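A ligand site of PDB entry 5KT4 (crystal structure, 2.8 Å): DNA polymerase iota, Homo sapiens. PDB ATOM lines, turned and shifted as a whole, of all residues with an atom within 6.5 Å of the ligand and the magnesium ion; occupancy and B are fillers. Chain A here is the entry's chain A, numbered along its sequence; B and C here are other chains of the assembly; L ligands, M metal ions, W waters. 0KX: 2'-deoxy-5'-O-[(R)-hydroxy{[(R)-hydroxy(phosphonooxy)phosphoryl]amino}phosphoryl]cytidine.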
ATOM      1  N   ASP A  59      24.829  -7.319  27.070  1.00  0.00           N
ATOM      2  CA  ASP A  59      23.758  -8.190  26.597  1.00  0.00           C
ATOM      3  C   ASP A  59      24.133  -9.609  26.944  1.00  0.00           C
ATOM      4  O   ASP A  59      25.179 -10.099  26.520  1.00  0.00           O
ATOM      5  CB  ASP A  59      23.549  -8.019  25.090  1.00  0.00           C
ATOM      6  CG  ASP A  59      22.374  -8.841  24.557  1.00  0.00           C
ATOM      7  OD1 ASP A  59      21.651  -8.319  23.687  1.00  0.00           O
ATOM      8  OD2 ASP A  59      22.181  -9.991  24.987  1.00  0.00           O
ATOM      9  N   LEU A  60      23.269 -10.295  27.694  1.00  0.00           N
ATOM     10  CA  LEU A  60      23.584 -11.633  28.176  1.00  0.00           C
ATOM     11  C   LEU A  60      23.425 -12.664  27.066  1.00  0.00           C
ATOM     12  O   LEU A  60      22.534 -12.559  26.215  1.00  0.00           O
ATOM     13  CB  LEU A  60      22.673 -11.977  29.358  1.00  0.00           C
ATOM     14  CG  LEU A  60      22.978 -11.142  30.604  1.00  0.00           C
ATOM     15  CD1 LEU A  60      21.823 -11.183  31.586  1.00  0.00           C
ATOM     16  CD2 LEU A  60      24.244 -11.659  31.253  1.00  0.00           C
ATOM     17  N   ASP A  61      24.298 -13.676  27.089  1.00  0.00           N
ATOM     18  CA  ASP A  61      24.217 -14.775  26.127  1.00  0.00           C
ATOM     19  C   ASP A  61      23.055 -15.685  26.483  1.00  0.00           C
ATOM     20  O   ASP A  61      22.932 -16.131  27.634  1.00  0.00           O
ATOM     21  CB  ASP A  61      25.518 -15.578  26.127  1.00  0.00           C
ATOM     22  CG  ASP A  61      26.751 -14.713  25.918  1.00  0.00           C
ATOM     23  OD1 ASP A  61      27.701 -14.848  26.728  1.00  0.00           O
ATOM     24  OD2 ASP A  61      26.797 -13.932  24.944  1.00  0.00           O
ATOM     25  N   CYS A  62      22.197 -15.983  25.484  1.00  0.00           N
ATOM     26  CA  CYS A  62      21.035 -16.855  25.604  1.00  0.00           C
ATOM     27  C   CYS A  62      20.483 -16.894  27.033  1.00  0.00           C
ATOM     28  O   CYS A  62      20.541 -17.933  27.699  1.00  0.00           O
ATOM     29  CB  CYS A  62      21.360 -18.272  25.127  1.00  0.00           C
ATOM     30  SG  CYS A  62      22.875 -18.969  25.821  1.00  0.00           S
ATOM     31  N   PHE A  63      19.952 -15.754  27.482  1.00  0.00           N
ATOM     32  CA  PHE A  63      19.728 -15.514  28.902  1.00  0.00           C
ATOM     33  C   PHE A  63      18.935 -16.640  29.567  1.00  0.00           C
ATOM     34  O   PHE A  63      19.423 -17.313  30.483  1.00  0.00           O
ATOM     35  CB  PHE A  63      19.027 -14.169  29.075  1.00  0.00           C
ATOM     36  CG  PHE A  63      18.786 -13.784  30.501  1.00  0.00           C
ATOM     37  CD1 PHE A  63      19.760 -13.973  31.458  1.00  0.00           C
ATOM     38  CD2 PHE A  63      17.571 -13.225  30.878  1.00  0.00           C
ATOM     39  CE1 PHE A  63      19.530 -13.628  32.778  1.00  0.00           C
ATOM     40  CE2 PHE A  63      17.335 -12.873  32.183  1.00  0.00           C
ATOM     41  CZ  PHE A  63      18.318 -13.069  33.140  1.00  0.00           C
ATOM     42  N   TYR A  64      17.695 -16.866  29.108  1.00  0.00           N
ATOM     43  CA  TYR A  64      16.845 -17.880  29.714  1.00  0.00           C
ATOM     44  C   TYR A  64      17.526 -19.250  29.709  1.00  0.00           C
ATOM     45  O   TYR A  64      17.545 -19.952  30.730  1.00  0.00           O
ATOM     46  CB  TYR A  64      15.498 -17.967  28.989  1.00  0.00           C
ATOM     47  CG  TYR A  64      14.599 -16.755  29.143  1.00  0.00           C
ATOM     48  CD1 TYR A  64      14.986 -15.644  29.896  1.00  0.00           C
ATOM     49  CD2 TYR A  64      13.340 -16.719  28.540  1.00  0.00           C
ATOM     50  CE1 TYR A  64      14.164 -14.549  30.040  1.00  0.00           C
ATOM     51  CE2 TYR A  64      12.501 -15.629  28.681  1.00  0.00           C
ATOM     52  CZ  TYR A  64      12.922 -14.542  29.425  1.00  0.00           C
ATOM     53  OH  TYR A  64      12.099 -13.448  29.569  1.00  0.00           O
ATOM     54  N   ALA A  65      18.095 -19.630  28.565  1.00  0.00           N
ATOM     55  CA  ALA A  65      18.799 -20.901  28.480  1.00  0.00           C
ATOM     56  C   ALA A  65      19.950 -20.952  29.473  1.00  0.00           C
ATOM     57  O   ALA A  65      20.181 -21.983  30.116  1.00  0.00           O
ATOM     58  CB  ALA A  65      19.305 -21.120  27.062  1.00  0.00           C
ATOM     59  N   GLN A  84       7.970 -21.340  25.229  1.00  0.00           N
ATOM     60  CA  GLN A  84       6.767 -20.703  25.751  1.00  0.00           C
ATOM     61  C   GLN A  84       5.654 -20.954  24.754  1.00  0.00           C
ATOM     62  O   GLN A  84       5.704 -20.449  23.628  1.00  0.00           O
ATOM     63  CB  GLN A  84       6.977 -19.199  25.978  1.00  0.00           C
ATOM     64  CG  GLN A  84       7.921 -18.876  27.121  1.00  0.00           C
ATOM     65  CD  GLN A  84       8.225 -17.389  27.220  1.00  0.00           C
ATOM     66  OE1 GLN A  84       8.125 -16.651  26.244  1.00  0.00           O
ATOM     67  NE2 GLN A  84       8.603 -16.948  28.423  1.00  0.00           N
ATOM     68  N   LEU A  87       6.427 -21.672  20.932  1.00  0.00           N
ATOM     69  CA  LEU A  87       7.554 -20.876  20.490  1.00  0.00           C
ATOM     70  C   LEU A  87       8.798 -21.227  21.287  1.00  0.00           C
ATOM     71  O   LEU A  87       8.761 -21.260  22.520  1.00  0.00           O
ATOM     72  CB  LEU A  87       7.242 -19.379  20.619  1.00  0.00           C
ATOM     73  CG  LEU A  87       8.152 -18.394  19.894  1.00  0.00           C
ATOM     74  CD1 LEU A  87       8.088 -18.614  18.392  1.00  0.00           C
ATOM     75  CD2 LEU A  87       7.794 -16.946  20.244  1.00  0.00           C
ATOM     76  N   VAL A  89      11.827 -19.707  22.511  1.00  0.00           N
ATOM     77  CA  VAL A  89      12.115 -18.285  22.650  1.00  0.00           C
ATOM     78  C   VAL A  89      13.617 -18.024  22.642  1.00  0.00           C
ATOM     79  O   VAL A  89      14.058 -16.939  22.251  1.00  0.00           O
ATOM     80  CB  VAL A  89      11.401 -17.740  23.901  1.00  0.00           C
ATOM     81  CG1 VAL A  89      12.297 -17.810  25.140  1.00  0.00           C
ATOM     82  CG2 VAL A  89      10.882 -16.342  23.652  1.00  0.00           C
ATOM     83  N   THR A  90      14.417 -19.004  23.047  1.00  0.00           N
ATOM     84  CA  THR A  90      15.873 -18.898  22.988  1.00  0.00           C
ATOM     85  C   THR A  90      16.454 -20.296  23.161  1.00  0.00           C
ATOM     86  O   THR A  90      15.758 -21.231  23.570  1.00  0.00           O
ATOM     87  CB  THR A  90      16.413 -17.940  24.051  1.00  0.00           C
ATOM     88  OG1 THR A  90      17.803 -17.690  23.810  1.00  0.00           O
ATOM     89  CG2 THR A  90      16.244 -18.532  25.443  1.00  0.00           C
ATOM     90  N   CYS A  91      17.727 -20.436  22.834  1.00  0.00           N
ATOM     91  CA  CYS A  91      18.387 -21.736  22.891  1.00  0.00           C
ATOM     92  C   CYS A  91      19.869 -21.537  23.130  1.00  0.00           C
ATOM     93  O   CYS A  91      20.407 -20.451  22.934  1.00  0.00           O
ATOM     94  CB  CYS A  91      18.157 -22.533  21.600  1.00  0.00           C
ATOM     95  SG  CYS A  91      18.904 -21.776  20.145  1.00  0.00           S
ATOM     96  N   LYS A 102      16.410 -18.234  17.401  1.00  0.00           N
ATOM     97  CA  LYS A 102      15.556 -17.595  18.381  1.00  0.00           C
ATOM     98  C   LYS A 102      14.178 -17.313  17.790  1.00  0.00           C
ATOM     99  O   LYS A 102      14.056 -16.907  16.636  1.00  0.00           O
ATOM    100  CB  LYS A 102      16.202 -16.308  18.891  1.00  0.00           C
ATOM    101  CG  LYS A 102      17.473 -16.556  19.694  1.00  0.00           C
ATOM    102  CD  LYS A 102      18.175 -15.269  20.091  1.00  0.00           C
ATOM    103  CE  LYS A 102      18.927 -14.649  18.914  1.00  0.00           C
ATOM    104  NZ  LYS A 102      19.591 -13.378  19.312  1.00  0.00           N
ATOM    105  N   LEU A 103      13.133 -17.545  18.594  1.00  0.00           N
ATOM    106  CA  LEU A 103      11.751 -17.312  18.196  1.00  0.00           C
ATOM    107  C   LEU A 103      11.338 -18.238  17.047  1.00  0.00           C
ATOM    108  O   LEU A 103      10.558 -17.858  16.173  1.00  0.00           O
ATOM    109  CB  LEU A 103      11.511 -15.839  17.821  1.00  0.00           C
ATOM    110  CG  LEU A 103      11.929 -14.796  18.858  1.00  0.00           C
ATOM    111  CD1 LEU A 103      11.743 -13.385  18.312  1.00  0.00           C
ATOM    112  CD2 LEU A 103      11.155 -14.972  20.150  1.00  0.00           C
ATOM    113  N   LEU A 124       8.615 -16.374  34.425  1.00  0.00           N
ATOM    114  CA  LEU A 124       9.789 -15.509  34.357  1.00  0.00           C
ATOM    115  C   LEU A 124      10.378 -15.191  35.722  1.00  0.00           C
ATOM    116  O   LEU A 124      11.163 -14.249  35.842  1.00  0.00           O
ATOM    117  CB  LEU A 124       9.455 -14.213  33.628  1.00  0.00           C
ATOM    118  CG  LEU A 124       8.697 -14.296  32.303  1.00  0.00           C
ATOM    119  CD1 LEU A 124       8.584 -12.909  31.653  1.00  0.00           C
ATOM    120  CD2 LEU A 124       9.347 -15.282  31.344  1.00  0.00           C
ATOM    121  N   PHE A 150      15.063  -7.832  29.976  1.00  0.00           N
ATOM    122  CA  PHE A 150      15.598  -8.509  31.137  1.00  0.00           C
ATOM    123  C   PHE A 150      17.109  -8.664  31.077  1.00  0.00           C
ATOM    124  O   PHE A 150      17.743  -8.817  32.129  1.00  0.00           O
ATOM    125  CB  PHE A 150      14.944  -9.886  31.305  1.00  0.00           C
ATOM    126  CG  PHE A 150      13.588  -9.841  31.955  1.00  0.00           C
ATOM    127  CD1 PHE A 150      12.937 -11.013  32.298  1.00  0.00           C
ATOM    128  CD2 PHE A 150      12.949  -8.632  32.215  1.00  0.00           C
ATOM    129  CE1 PHE A 150      11.691 -10.999  32.900  1.00  0.00           C
ATOM    130  CE2 PHE A 150      11.700  -8.607  32.810  1.00  0.00           C
ATOM    131  CZ  PHE A 150      11.078  -9.791  33.150  1.00  0.00           C
ATOM    132  N   ASP A 151      17.717  -8.635  29.893  1.00  0.00           N
ATOM    133  CA  ASP A 151      19.103  -9.069  29.760  1.00  0.00           C
ATOM    134  C   ASP A 151      20.044  -8.006  29.212  1.00  0.00           C
ATOM    135  O   ASP A 151      21.212  -8.322  28.938  1.00  0.00           O
ATOM    136  CB  ASP A 151      19.179 -10.312  28.879  1.00  0.00           C
ATOM    137  CG  ASP A 151      19.178  -9.979  27.392  1.00  0.00           C
ATOM    138  OD1 ASP A 151      18.413  -9.087  26.985  1.00  0.00           O
ATOM    139  OD2 ASP A 151      19.949 -10.613  26.650  1.00  0.00           O
ATOM    140  N   GLU A 152      19.604  -6.756  29.039  1.00  0.00           N
ATOM    141  CA  GLU A 152      20.489  -5.727  28.524  1.00  0.00           C
ATOM    142  C   GLU A 152      20.588  -4.553  29.490  1.00  0.00           C
ATOM    143  O   GLU A 152      19.607  -4.213  30.152  1.00  0.00           O
ATOM    144  CB  GLU A 152      20.038  -5.268  27.139  1.00  0.00           C
ATOM    145  CG  GLU A 152      20.314  -6.318  26.077  1.00  0.00           C
ATOM    146  CD  GLU A 152      19.694  -6.005  24.735  1.00  0.00           C
ATOM    147  OE1 GLU A 152      19.636  -4.820  24.379  1.00  0.00           O
ATOM    148  OE2 GLU A 152      19.275  -6.961  24.050  1.00  0.00           O
ATOM    149  N   LYS A 239      30.260 -12.692  19.216  1.00  0.00           N
ATOM    150  CA  LYS A 239      29.408 -13.484  20.103  1.00  0.00           C
ATOM    151  C   LYS A 239      29.830 -14.945  20.100  1.00  0.00           C
ATOM    152  O   LYS A 239      30.246 -15.473  19.058  1.00  0.00           O
ATOM    153  CB  LYS A 239      27.941 -13.352  19.683  1.00  0.00           C
ATOM    154  CG  LYS A 239      27.252 -12.105  20.208  1.00  0.00           C
ATOM    155  CD  LYS A 239      25.896 -11.892  19.542  1.00  0.00           C
ATOM    156  CE  LYS A 239      24.999 -13.117  19.658  1.00  0.00           C
ATOM    157  NZ  LYS A 239      23.613 -12.854  19.188  1.00  0.00           N
ATOM    158  N   PRO A 240      29.720 -15.623  21.257  1.00  0.00           N
ATOM    159  CA  PRO A 240      29.289 -15.051  22.533  1.00  0.00           C
ATOM    160  C   PRO A 240      30.447 -14.784  23.487  1.00  0.00           C
ATOM    161  O   PRO A 240      31.600 -15.110  23.175  1.00  0.00           O
ATOM    162  CB  PRO A 240      28.382 -16.132  23.093  1.00  0.00           C
ATOM    163  CG  PRO A 240      29.035 -17.397  22.634  1.00  0.00           C
ATOM    164  CD  PRO A 240      29.696 -17.095  21.296  1.00  0.00           C
ATOM    165  P    DC B   7      15.868  -4.702  20.654  1.00  0.00           P
ATOM    166  OP1  DC B   7      17.296  -4.579  20.282  1.00  0.00           O
ATOM    167  OP2  DC B   7      14.828  -4.978  19.632  1.00  0.00           O
ATOM    168  O5'  DC B   7      15.731  -5.801  21.803  1.00  0.00           O
ATOM    169  C5'  DC B   7      16.489  -5.664  22.985  1.00  0.00           C
ATOM    170  C4'  DC B   7      15.966  -6.584  24.067  1.00  0.00           C
ATOM    171  O4'  DC B   7      14.604  -6.251  24.368  1.00  0.00           O
ATOM    172  C3'  DC B   7      15.916  -8.044  23.680  1.00  0.00           C
ATOM    173  O3'  DC B   7      17.200  -8.635  23.844  1.00  0.00           O
ATOM    174  C2'  DC B   7      14.928  -8.586  24.712  1.00  0.00           C
ATOM    175  C1'  DC B   7      13.953  -7.407  24.868  1.00  0.00           C
ATOM    176  N1   DC B   7      12.678  -7.588  24.118  1.00  0.00           N
ATOM    177  C2   DC B   7      11.711  -8.459  24.628  1.00  0.00           C
ATOM    178  O2   DC B   7      11.942  -9.057  25.683  1.00  0.00           O
ATOM    179  N3   DC B   7      10.546  -8.614  23.945  1.00  0.00           N
ATOM    180  C4   DC B   7      10.346  -7.941  22.810  1.00  0.00           C
ATOM    181  N4   DC B   7       9.192  -8.126  22.157  1.00  0.00           N
ATOM    182  C5   DC B   7      11.329  -7.053  22.281  1.00  0.00           C
ATOM    183  C6   DC B   7      12.464  -6.902  22.966  1.00  0.00           C
ATOM    184  P    DG C   3       1.443 -17.524  20.853  1.00  0.00           P
ATOM    185  OP1  DG C   3       0.276 -18.433  20.822  1.00  0.00           O
ATOM    186  OP2  DG C   3       1.265 -16.061  20.681  1.00  0.00           O
ATOM    187  O5'  DG C   3       2.219 -17.656  22.237  1.00  0.00           O
ATOM    188  C5'  DG C   3       3.587 -17.260  22.288  1.00  0.00           C
ATOM    189  C4'  DG C   3       4.158 -17.462  23.674  1.00  0.00           C
ATOM    190  O4'  DG C   3       5.505 -16.944  23.723  1.00  0.00           O
ATOM    191  C3'  DG C   3       3.417 -16.736  24.765  1.00  0.00           C
ATOM    192  O3'  DG C   3       3.606 -17.405  25.992  1.00  0.00           O
ATOM    193  C2'  DG C   3       4.092 -15.367  24.751  1.00  0.00           C
ATOM    194  C1'  DG C   3       5.545 -15.767  24.514  1.00  0.00           C
ATOM    195  N9   DG C   3       6.360 -14.768  23.816  1.00  0.00           N
ATOM    196  C8   DG C   3       7.632 -14.373  24.153  1.00  0.00           C
ATOM    197  N7   DG C   3       8.139 -13.486  23.348  1.00  0.00           N
ATOM    198  C5   DG C   3       7.154 -13.273  22.404  1.00  0.00           C
ATOM    199  C6   DG C   3       7.144 -12.414  21.279  1.00  0.00           C
ATOM    200  O6   DG C   3       8.026 -11.647  20.891  1.00  0.00           O
ATOM    201  N1   DG C   3       5.942 -12.505  20.577  1.00  0.00           N
ATOM    202  C2   DG C   3       4.891 -13.319  20.924  1.00  0.00           C
ATOM    203  N2   DG C   3       3.814 -13.268  20.121  1.00  0.00           N
ATOM    204  N3   DG C   3       4.887 -14.131  21.968  1.00  0.00           N
ATOM    205  C4   DG C   3       6.047 -14.062  22.663  1.00  0.00           C
ATOM    206  P    DG C   4       2.667 -17.073  27.242  1.00  0.00           P
ATOM    207  OP1  DG C   4       2.508 -18.305  28.042  1.00  0.00           O
ATOM    208  OP2  DG C   4       1.481 -16.364  26.693  1.00  0.00           O
ATOM    209  O5'  DG C   4       3.526 -16.040  28.084  1.00  0.00           O
ATOM    210  C5'  DG C   4       4.764 -16.462  28.651  1.00  0.00           C
ATOM    211  C4'  DG C   4       5.523 -15.271  29.185  1.00  0.00           C
ATOM    212  O4'  DG C   4       6.085 -14.525  28.057  1.00  0.00           O
ATOM    213  C3'  DG C   4       4.670 -14.271  29.967  1.00  0.00           C
ATOM    214  O3'  DG C   4       5.374 -13.809  31.130  1.00  0.00           O
ATOM    215  C2'  DG C   4       4.467 -13.143  28.957  1.00  0.00           C
ATOM    216  C1'  DG C   4       5.817 -13.169  28.271  1.00  0.00           C
ATOM    217  N9   DG C   4       5.842 -12.442  27.007  1.00  0.00           N
ATOM    218  C8   DG C   4       4.827 -12.315  26.087  1.00  0.00           C
ATOM    219  N7   DG C   4       5.140 -11.576  25.063  1.00  0.00           N
ATOM    220  C5   DG C   4       6.454 -11.176  25.327  1.00  0.00           C
ATOM    221  C6   DG C   4       7.329 -10.357  24.580  1.00  0.00           C
ATOM    222  O6   DG C   4       7.135  -9.799  23.487  1.00  0.00           O
ATOM    223  N1   DG C   4       8.567 -10.214  25.217  1.00  0.00           N
ATOM    224  C2   DG C   4       8.900 -10.783  26.418  1.00  0.00           C
ATOM    225  N2   DG C   4      10.122 -10.545  26.888  1.00  0.00           N
ATOM    226  N3   DG C   4       8.084 -11.550  27.117  1.00  0.00           N
ATOM    227  C4   DG C   4       6.884 -11.700  26.523  1.00  0.00           C
HETATM  228  PG  0KX L   1      21.658 -13.674  22.519  1.00  0.00           P
HETATM  229  O1G 0KX L   1      21.546 -12.383  23.301  1.00  0.00           O
HETATM  230  O2G 0KX L   1      21.399 -13.514  21.040  1.00  0.00           O
HETATM  231  O3G 0KX L   1      22.889 -14.486  22.852  1.00  0.00           O
HETATM  232  PB  0KX L   1      19.222 -14.161  23.957  1.00  0.00           P
HETATM  233  O1B 0KX L   1      18.540 -15.447  24.344  1.00  0.00           O
HETATM  234  O2B 0KX L   1      19.740 -13.289  25.066  1.00  0.00           O
HETATM  235  O3B 0KX L   1      20.465 -14.626  23.035  1.00  0.00           O
HETATM  236  PA  0KX L   1      17.704 -11.636  23.509  1.00  0.00           P
HETATM  237  O1A 0KX L   1      18.948 -10.943  24.030  1.00  0.00           O
HETATM  238  O2A 0KX L   1      16.957 -10.948  22.386  1.00  0.00           O
HETATM  239  N3A 0KX L   1      18.106 -13.256  22.928  1.00  0.00           N
HETATM  240  O5' 0KX L   1      16.640 -11.728  24.713  1.00  0.00           O
HETATM  241  C5' 0KX L   1      16.997 -12.143  26.027  1.00  0.00           C
HETATM  242  C4' 0KX L   1      15.899 -13.045  26.572  1.00  0.00           C
HETATM  243  O4' 0KX L   1      14.629 -12.404  26.482  1.00  0.00           O
HETATM  244  C3' 0KX L   1      15.792 -14.331  25.769  1.00  0.00           C
HETATM  245  O3' 0KX L   1      16.513 -15.382  26.426  1.00  0.00           O
HETATM  246  C2' 0KX L   1      14.309 -14.643  25.729  1.00  0.00           C
HETATM  247  C1' 0KX L   1      13.621 -13.330  26.076  1.00  0.00           C
HETATM  248  N1  0KX L   1      12.937 -12.804  24.890  1.00  0.00           N
HETATM  249  C2  0KX L   1      11.570 -13.094  24.696  1.00  0.00           C
HETATM  250  N3  0KX L   1      10.927 -12.611  23.603  1.00  0.00           N
HETATM  251  C4  0KX L   1      11.590 -11.854  22.699  1.00  0.00           C
HETATM  252  C5  0KX L   1      12.930 -11.569  22.881  1.00  0.00           C
HETATM  253  C6  0KX L   1      13.589 -12.058  23.999  1.00  0.00           C
HETATM  254  O2  0KX L   1      10.957 -13.783  25.530  1.00  0.00           O
HETATM  255  N4  0KX L   1      10.926 -11.382  21.609  1.00  0.00           N
HETATM  256 MG    MG M   1      20.930 -11.617  25.093  1.00  0.00          MG
HETATM  257  O   HOH W   1      21.166 -10.329  21.341  1.00  0.00           O
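OG1 of Thr 90 sits at hydrogen-bond distance from O1B of the ligand, 2.4 Å away.
NZ of Lys 102 is in salt-bridge range of O2G of the ligand.
O3' of DC 7 of chain B sits close to an oxygen (O2A) of the ligand, at 2.7 Å.
O6 of DG 3 of chain C is in hydrogen-bond range of a nitrogen (N4) of the ligand.
The side-chain amino group of Lys 239 lies within salt-bridge range of an oxygen (O2G) of the ligand, 3.0 Å away.
O3G of the ligand lies within hydrogen-bond range of N of Cys 62 (3.1 Å).
The backbone NH of Tyr 64 sits at hydrogen-bond distance from an oxygen (O3') of the ligand, 3.3 Å away.
N of Phe 63 sits at hydrogen-bond distance from O1B of the ligand (3.5 Å).
O2 of DC 7 of chain B sits close to N2 of DG 4 of chain C (2.6 Å).
O3' of DC 7 of chain B lies close to the side-chain carboxylate of Glu 152 (2.7 Å).
O4' of DG 4 of chain C lies close to OE1 of Gln 84 (3.5 Å).
Asp 61 touches the ligand.
CG2 of Val 89 touches O2 of the ligand, 3.2 Å away.
CD2 of Leu 103 touches N4 of the ligand, at 3.9 Å.
OE2 of Glu 152 touches O1A of the ligand, at 3.995 Å.
DG 4 of chain C touches the ligand (N2 to O2, 3.6 Å).
Hydrophobic or aromatic side chains that line the ligand: Phe 63, Tyr 64, Val 89 and Leu 103.
Of the 23 residues printed, 16 come within 4 Å of the ligand.
The nearest printed residue that does not touch the ligand is Gln 84 (4.1 Å).
Of the 23 residues printed, 3 come within 4 Å of the magnesium ion.
The magnesium ion is bound by an oxygen (O1G) of the ligand (2.0 Å), an oxygen (O2B) of the ligand (2.1 Å), the side-chain carboxylate (OD2) of Asp 59 (2.1 Å), the side-chain carboxylate (OD2) of Asp 151 (2.1 Å), the backbone carbonyl oxygen (O) of Leu 60 (2.2 Å) and an oxygen (O1A) of the ligand (2.3 Å).
Water W1 lies within hydrogen-bond range of the side-chain carboxylate (OD1) of Asp 59 (3.1 Å) and an oxygen (O2G) of the ligand (3.2 Å).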
